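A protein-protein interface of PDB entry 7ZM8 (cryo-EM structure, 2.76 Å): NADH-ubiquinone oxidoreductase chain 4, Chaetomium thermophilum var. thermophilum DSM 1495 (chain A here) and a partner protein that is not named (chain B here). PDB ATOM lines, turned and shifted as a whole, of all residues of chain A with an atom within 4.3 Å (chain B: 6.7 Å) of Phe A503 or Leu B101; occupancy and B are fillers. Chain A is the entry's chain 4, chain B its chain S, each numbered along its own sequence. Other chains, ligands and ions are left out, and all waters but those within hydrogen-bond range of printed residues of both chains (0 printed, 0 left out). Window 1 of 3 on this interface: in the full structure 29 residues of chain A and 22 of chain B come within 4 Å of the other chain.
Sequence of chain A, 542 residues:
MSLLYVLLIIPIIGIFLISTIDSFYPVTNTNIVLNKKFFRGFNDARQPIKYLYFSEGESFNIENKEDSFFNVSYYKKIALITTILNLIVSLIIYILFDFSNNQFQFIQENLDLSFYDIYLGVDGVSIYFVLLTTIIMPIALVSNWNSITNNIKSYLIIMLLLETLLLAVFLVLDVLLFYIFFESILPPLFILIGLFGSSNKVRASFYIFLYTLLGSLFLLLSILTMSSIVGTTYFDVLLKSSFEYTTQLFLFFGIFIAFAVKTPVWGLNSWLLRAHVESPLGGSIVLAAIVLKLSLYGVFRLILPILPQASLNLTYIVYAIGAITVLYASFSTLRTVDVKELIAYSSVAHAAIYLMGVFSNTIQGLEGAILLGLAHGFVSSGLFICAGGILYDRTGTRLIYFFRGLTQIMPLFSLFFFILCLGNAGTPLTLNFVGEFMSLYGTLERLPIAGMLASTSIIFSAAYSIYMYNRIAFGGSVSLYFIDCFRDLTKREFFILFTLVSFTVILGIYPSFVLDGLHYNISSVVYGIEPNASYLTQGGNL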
ATOM      1  N   ILE A 135      13.459 -15.175 -18.090  1.00  0.00           N
ATOM      2  CA  ILE A 135      12.374 -15.664 -17.197  1.00  0.00           C
ATOM      3  C   ILE A 135      12.198 -17.136 -17.539  1.00  0.00           C
ATOM      4  O   ILE A 135      11.854 -17.924 -16.660  1.00  0.00           O
ATOM      5  CB  ILE A 135      11.080 -14.837 -17.333  1.00  0.00           C
ATOM      6  CG1 ILE A 135      11.284 -13.384 -16.902  1.00  0.00           C
ATOM      7  CG2 ILE A 135       9.927 -15.486 -16.586  1.00  0.00           C
ATOM      8  CD1 ILE A 135      10.256 -12.432 -17.458  1.00  0.00           C
ATOM      9  N   PHE A 378       5.133 -18.168 -23.039  1.00  0.00           N
ATOM     10  CA  PHE A 378       4.654 -18.653 -21.751  1.00  0.00           C
ATOM     11  C   PHE A 378       3.750 -19.867 -21.903  1.00  0.00           C
ATOM     12  O   PHE A 378       3.872 -20.832 -21.144  1.00  0.00           O
ATOM     13  CB  PHE A 378       3.909 -17.544 -21.007  1.00  0.00           C
ATOM     14  CG  PHE A 378       4.739 -16.332 -20.723  1.00  0.00           C
ATOM     15  CD1 PHE A 378       5.851 -16.414 -19.912  1.00  0.00           C
ATOM     16  CD2 PHE A 378       4.396 -15.103 -21.253  1.00  0.00           C
ATOM     17  CE1 PHE A 378       6.610 -15.300 -19.648  1.00  0.00           C
ATOM     18  CE2 PHE A 378       5.152 -13.987 -20.991  1.00  0.00           C
ATOM     19  CZ  PHE A 378       6.257 -14.085 -20.187  1.00  0.00           C
ATOM     20  N   THR A 499       3.609 -20.072 -12.052  1.00  0.00           N
ATOM     21  CA  THR A 499       4.385 -18.918 -12.490  1.00  0.00           C
ATOM     22  C   THR A 499       4.145 -18.610 -13.961  1.00  0.00           C
ATOM     23  O   THR A 499       3.970 -17.448 -14.339  1.00  0.00           O
ATOM     24  CB  THR A 499       5.871 -19.166 -12.233  1.00  0.00           C
ATOM     25  OG1 THR A 499       6.070 -19.470 -10.850  1.00  0.00           O
ATOM     26  CG2 THR A 499       6.680 -17.947 -12.596  1.00  0.00           C
ATOM     27  N   LEU A 500       4.140 -19.639 -14.809  1.00  0.00           N
ATOM     28  CA  LEU A 500       3.915 -19.424 -16.234  1.00  0.00           C
ATOM     29  C   LEU A 500       2.495 -18.951 -16.514  1.00  0.00           C
ATOM     30  O   LEU A 500       2.284 -18.101 -17.384  1.00  0.00           O
ATOM     31  CB  LEU A 500       4.214 -20.704 -17.008  1.00  0.00           C
ATOM     32  CG  LEU A 500       5.682 -20.990 -17.315  1.00  0.00           C
ATOM     33  CD1 LEU A 500       5.820 -22.413 -17.770  1.00  0.00           C
ATOM     34  CD2 LEU A 500       6.217 -20.037 -18.367  1.00  0.00           C
ATOM     35  N   VAL A 501       1.509 -19.496 -15.801  1.00  0.00           N
ATOM     36  CA  VAL A 501       0.132 -19.040 -15.977  1.00  0.00           C
ATOM     37  C   VAL A 501      -0.022 -17.607 -15.486  1.00  0.00           C
ATOM     38  O   VAL A 501      -0.758 -16.812 -16.079  1.00  0.00           O
ATOM     39  CB  VAL A 501      -0.842 -20.002 -15.268  1.00  0.00           C
ATOM     40  CG1 VAL A 501      -2.227 -19.402 -15.170  1.00  0.00           C
ATOM     41  CG2 VAL A 501      -0.916 -21.325 -16.014  1.00  0.00           C
ATOM     42  N   SER A 502       0.673 -17.253 -14.402  1.00  0.00           N
ATOM     43  CA  SER A 502       0.563 -15.908 -13.843  1.00  0.00           C
ATOM     44  C   SER A 502       1.045 -14.849 -14.822  1.00  0.00           C
ATOM     45  O   SER A 502       0.421 -13.794 -14.956  1.00  0.00           O
ATOM     46  CB  SER A 502       1.352 -15.820 -12.539  1.00  0.00           C
ATOM     47  OG  SER A 502       0.803 -16.680 -11.563  1.00  0.00           O
ATOM     48  N   PHE A 503       2.166 -15.100 -15.496  1.00  0.00           N
ATOM     49  CA  PHE A 503       2.630 -14.174 -16.523  1.00  0.00           C
ATOM     50  C   PHE A 503       1.617 -14.075 -17.651  1.00  0.00           C
ATOM     51  O   PHE A 503       1.367 -12.992 -18.191  1.00  0.00           O
ATOM     52  CB  PHE A 503       3.980 -14.635 -17.064  1.00  0.00           C
ATOM     53  CG  PHE A 503       5.151 -14.050 -16.346  1.00  0.00           C
ATOM     54  CD1 PHE A 503       5.516 -12.731 -16.549  1.00  0.00           C
ATOM     55  CD2 PHE A 503       5.893 -14.817 -15.467  1.00  0.00           C
ATOM     56  CE1 PHE A 503       6.596 -12.190 -15.888  1.00  0.00           C
ATOM     57  CE2 PHE A 503       6.971 -14.279 -14.805  1.00  0.00           C
ATOM     58  CZ  PHE A 503       7.324 -12.965 -15.015  1.00  0.00           C
ATOM     59  N   THR A 504       1.011 -15.195 -18.058  1.00  0.00           N
ATOM     60  CA  THR A 504       0.079 -15.166 -19.222  1.00  0.00           C
ATOM     61  C   THR A 504      -1.172 -14.354 -18.889  1.00  0.00           C
ATOM     62  O   THR A 504      -1.668 -13.666 -19.793  1.00  0.00           O
ATOM     63  CB  THR A 504      -0.416 -16.555 -19.657  1.00  0.00           C
ATOM     64  OG1 THR A 504      -1.393 -17.049 -18.743  1.00  0.00           O
ATOM     65  CG2 THR A 504       0.681 -17.577 -19.839  1.00  0.00           C
ATOM     66  N   VAL A 505      -1.667 -14.435 -17.651  1.00  0.00           N
ATOM     67  CA  VAL A 505      -2.932 -13.773 -17.342  1.00  0.00           C
ATOM     68  C   VAL A 505      -2.730 -12.303 -16.999  1.00  0.00           C
ATOM     69  O   VAL A 505      -3.475 -11.441 -17.470  1.00  0.00           O
ATOM     70  CB  VAL A 505      -3.652 -14.526 -16.205  1.00  0.00           C
ATOM     71  CG1 VAL A 505      -5.014 -13.916 -15.948  1.00  0.00           C
ATOM     72  CG2 VAL A 505      -3.798 -15.988 -16.561  1.00  0.00           C
ATOM     73  N   ILE A 506      -1.735 -11.997 -16.169  1.00  0.00           N
ATOM     74  CA  ILE A 506      -1.495 -10.616 -15.759  1.00  0.00           C
ATOM     75  C   ILE A 506      -1.162  -9.752 -16.965  1.00  0.00           C
ATOM     76  O   ILE A 506      -1.654  -8.626 -17.097  1.00  0.00           O
ATOM     77  CB  ILE A 506      -0.379 -10.567 -14.700  1.00  0.00           C
ATOM     78  CG1 ILE A 506      -0.812 -11.318 -13.443  1.00  0.00           C
ATOM     79  CG2 ILE A 506      -0.016  -9.139 -14.363  1.00  0.00           C
ATOM     80  CD1 ILE A 506       0.304 -11.544 -12.460  1.00  0.00           C
ATOM     81  N   LEU A 507      -0.321 -10.263 -17.865  1.00  0.00           N
ATOM     82  CA  LEU A 507      -0.007  -9.540 -19.089  1.00  0.00           C
ATOM     83  C   LEU A 507      -1.196  -9.456 -20.028  1.00  0.00           C
ATOM     84  O   LEU A 507      -1.247  -8.545 -20.855  1.00  0.00           O
ATOM     85  CB  LEU A 507       1.176 -10.195 -19.801  1.00  0.00           C
ATOM     86  CG  LEU A 507       2.551  -9.704 -19.345  1.00  0.00           C
ATOM     87  CD1 LEU A 507       3.656 -10.504 -19.989  1.00  0.00           C
ATOM     88  CD2 LEU A 507       2.707  -8.234 -19.657  1.00  0.00           C
ATOM     89  N   GLY B  96      14.932 -15.785  -4.803  1.00  0.00           N
ATOM     90  CA  GLY B  96      15.581 -15.092  -5.890  1.00  0.00           C
ATOM     91  C   GLY B  96      14.668 -14.824  -7.061  1.00  0.00           C
ATOM     92  O   GLY B  96      14.574 -13.688  -7.526  1.00  0.00           O
ATOM     93  N   PHE B  97      13.995 -15.861  -7.554  1.00  0.00           N
ATOM     94  CA  PHE B  97      13.139 -15.686  -8.720  1.00  0.00           C
ATOM     95  C   PHE B  97      11.926 -14.835  -8.377  1.00  0.00           C
ATOM     96  O   PHE B  97      11.704 -13.783  -8.980  1.00  0.00           O
ATOM     97  CB  PHE B  97      12.716 -17.042  -9.281  1.00  0.00           C
ATOM     98  CG  PHE B  97      11.904 -16.943 -10.537  1.00  0.00           C
ATOM     99  CD1 PHE B  97      12.522 -16.798 -11.764  1.00  0.00           C
ATOM    100  CD2 PHE B  97      10.524 -16.986 -10.489  1.00  0.00           C
ATOM    101  CE1 PHE B  97      11.779 -16.703 -12.915  1.00  0.00           C
ATOM    102  CE2 PHE B  97       9.781 -16.887 -11.635  1.00  0.00           C
ATOM    103  CZ  PHE B  97      10.406 -16.742 -12.849  1.00  0.00           C
ATOM    104  N   TRP B  98      11.136 -15.260  -7.394  1.00  0.00           N
ATOM    105  CA  TRP B  98       9.949 -14.485  -7.056  1.00  0.00           C
ATOM    106  C   TRP B  98      10.315 -13.202  -6.332  1.00  0.00           C
ATOM    107  O   TRP B  98       9.745 -12.147  -6.619  1.00  0.00           O
ATOM    108  CB  TRP B  98       8.980 -15.323  -6.233  1.00  0.00           C
ATOM    109  CG  TRP B  98       8.092 -16.125  -7.107  1.00  0.00           C
ATOM    110  CD1 TRP B  98       8.179 -17.456  -7.362  1.00  0.00           C
ATOM    111  CD2 TRP B  98       6.997 -15.637  -7.886  1.00  0.00           C
ATOM    112  NE1 TRP B  98       7.195 -17.836  -8.236  1.00  0.00           N
ATOM    113  CE2 TRP B  98       6.455 -16.735  -8.572  1.00  0.00           C
ATOM    114  CE3 TRP B  98       6.415 -14.379  -8.059  1.00  0.00           C
ATOM    115  CZ2 TRP B  98       5.361 -16.614  -9.417  1.00  0.00           C
ATOM    116  CZ3 TRP B  98       5.335 -14.261  -8.898  1.00  0.00           C
ATOM    117  CH2 TRP B  98       4.817 -15.371  -9.568  1.00  0.00           C
ATOM    118  N   GLY B  99      11.293 -13.259  -5.427  1.00  0.00           N
ATOM    119  CA  GLY B  99      11.710 -12.053  -4.732  1.00  0.00           C
ATOM    120  C   GLY B  99      12.136 -10.952  -5.683  1.00  0.00           C
ATOM    121  O   GLY B  99      11.845  -9.777  -5.457  1.00  0.00           O
ATOM    122  N   SER B 100      12.817 -11.318  -6.768  1.00  0.00           N
ATOM    123  CA  SER B 100      13.217 -10.327  -7.757  1.00  0.00           C
ATOM    124  C   SER B 100      12.012  -9.679  -8.423  1.00  0.00           C
ATOM    125  O   SER B 100      12.065  -8.498  -8.777  1.00  0.00           O
ATOM    126  CB  SER B 100      14.121 -10.970  -8.806  1.00  0.00           C
ATOM    127  OG  SER B 100      14.806  -9.991  -9.566  1.00  0.00           O
ATOM    128  N   LEU B 101      10.925 -10.431  -8.609  1.00  0.00           N
ATOM    129  CA  LEU B 101       9.741  -9.888  -9.271  1.00  0.00           C
ATOM    130  C   LEU B 101       8.964  -8.928  -8.377  1.00  0.00           C
ATOM    131  O   LEU B 101       8.446  -7.921  -8.865  1.00  0.00           O
ATOM    132  CB  LEU B 101       8.847 -11.022  -9.764  1.00  0.00           C
ATOM    133  CG  LEU B 101       9.127 -11.577 -11.165  1.00  0.00           C
ATOM    134  CD1 LEU B 101      10.452 -12.287 -11.280  1.00  0.00           C
ATOM    135  CD2 LEU B 101       8.009 -12.522 -11.554  1.00  0.00           C
ATOM    136  N   ILE B 102       8.838  -9.222  -7.079  1.00  0.00           N
ATOM    137  CA  ILE B 102       8.226  -8.239  -6.186  1.00  0.00           C
ATOM    138  C   ILE B 102       9.088  -6.988  -6.089  1.00  0.00           C
ATOM    139  O   ILE B 102       8.575  -5.863  -6.114  1.00  0.00           O
ATOM    140  CB  ILE B 102       7.929  -8.820  -4.788  1.00  0.00           C
ATOM    141  CG1 ILE B 102       6.898  -9.955  -4.831  1.00  0.00           C
ATOM    142  CG2 ILE B 102       7.469  -7.728  -3.837  1.00  0.00           C
ATOM    143  CD1 ILE B 102       7.437 -11.324  -5.027  1.00  0.00           C
ATOM    144  N   VAL B 103      10.402  -7.155  -5.968  1.00  0.00           N
ATOM    145  CA  VAL B 103      11.285  -5.995  -5.913  1.00  0.00           C
ATOM    146  C   VAL B 103      11.263  -5.247  -7.241  1.00  0.00           C
ATOM    147  O   VAL B 103      11.377  -4.017  -7.276  1.00  0.00           O
ATOM    148  CB  VAL B 103      12.705  -6.431  -5.514  1.00  0.00           C
ATOM    149  CG1 VAL B 103      13.661  -5.253  -5.558  1.00  0.00           C
ATOM    150  CG2 VAL B 103      12.682  -7.021  -4.130  1.00  0.00           C
ATOM    151  N   PHE B 104      11.121  -5.972  -8.351  1.00  0.00           N
ATOM    152  CA  PHE B 104      10.934  -5.314  -9.638  1.00  0.00           C
ATOM    153  C   PHE B 104       9.594  -4.597  -9.697  1.00  0.00           C
ATOM    154  O   PHE B 104       9.490  -3.515 -10.282  1.00  0.00           O
ATOM    155  CB  PHE B 104      11.051  -6.332 -10.771  1.00  0.00           C
ATOM    156  CG  PHE B 104      10.582  -5.814 -12.096  1.00  0.00           C
ATOM    157  CD1 PHE B 104      11.396  -5.012 -12.864  1.00  0.00           C
ATOM    158  CD2 PHE B 104       9.318  -6.122 -12.565  1.00  0.00           C
ATOM    159  CE1 PHE B 104      10.964  -4.534 -14.069  1.00  0.00           C
ATOM    160  CE2 PHE B 104       8.880  -5.637 -13.767  1.00  0.00           C
ATOM    161  CZ  PHE B 104       9.702  -4.848 -14.519  1.00  0.00           C
ATOM    162  N   ALA B 105       8.555  -5.189  -9.109  1.00  0.00           N
ATOM    163  CA  ALA B 105       7.234  -4.572  -9.127  1.00  0.00           C
ATOM    164  C   ALA B 105       7.201  -3.281  -8.317  1.00  0.00           C
ATOM    165  O   ALA B 105       6.627  -2.281  -8.759  1.00  0.00           O
ATOM    166  CB  ALA B 105       6.190  -5.556  -8.608  1.00  0.00           C
ATOM    167  N   ILE B 106       7.808  -3.278  -7.131  1.00  0.00           N
ATOM    168  CA  ILE B 106       7.808  -2.063  -6.326  1.00  0.00           C
ATOM    169  C   ILE B 106       8.670  -0.990  -6.978  1.00  0.00           C
ATOM    170  O   ILE B 106       8.339   0.201  -6.934  1.00  0.00           O
ATOM    171  CB  ILE B 106       8.247  -2.366  -4.881  1.00  0.00           C
ATOM    172  CG1 ILE B 106       8.072  -1.125  -4.007  1.00  0.00           C
ATOM    173  CG2 ILE B 106       9.675  -2.850  -4.824  1.00  0.00           C
ATOM    174  CD1 ILE B 106       8.150  -1.408  -2.526  1.00  0.00           C
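The side-chain hydroxyl (OG1) of Thr A499 sits close to the indole nitrogen (NE1) of Trp B98.
Of the printed residues of chain B, Ile A135 touches Phe B97.
Of the printed residues of chain B, Thr A499 touches Phe B97 and Trp B98.
Phe A503 touches just one residue of chain B: Leu B101.
Printed residues of chain A within 4 Å of Phe B97: Ile A135 and Thr A499.
Of the printed residues of chain A, Trp B98 touches Thr A499.
Ile B106 touches none of the printed residues of chain A.
Among the printed residues, merely in contact across the chains: Ile A135 with Phe B97, Thr A499 with Phe B97 and Phe A503 with Leu B101.
Printed residues of chain A that touch a printed residue of chain B: Ile A135, Thr A499 and Phe A503.
Along chain A the printed residues that touch a printed residue of chain B span positions 135 to 503.
Among the printed residues, 4 pairs touch across the chains.
Among the printed residues, no Asp or Glu carboxylate lies within 4 Å of a Lys or Arg side-chain nitrogen of the other chain.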
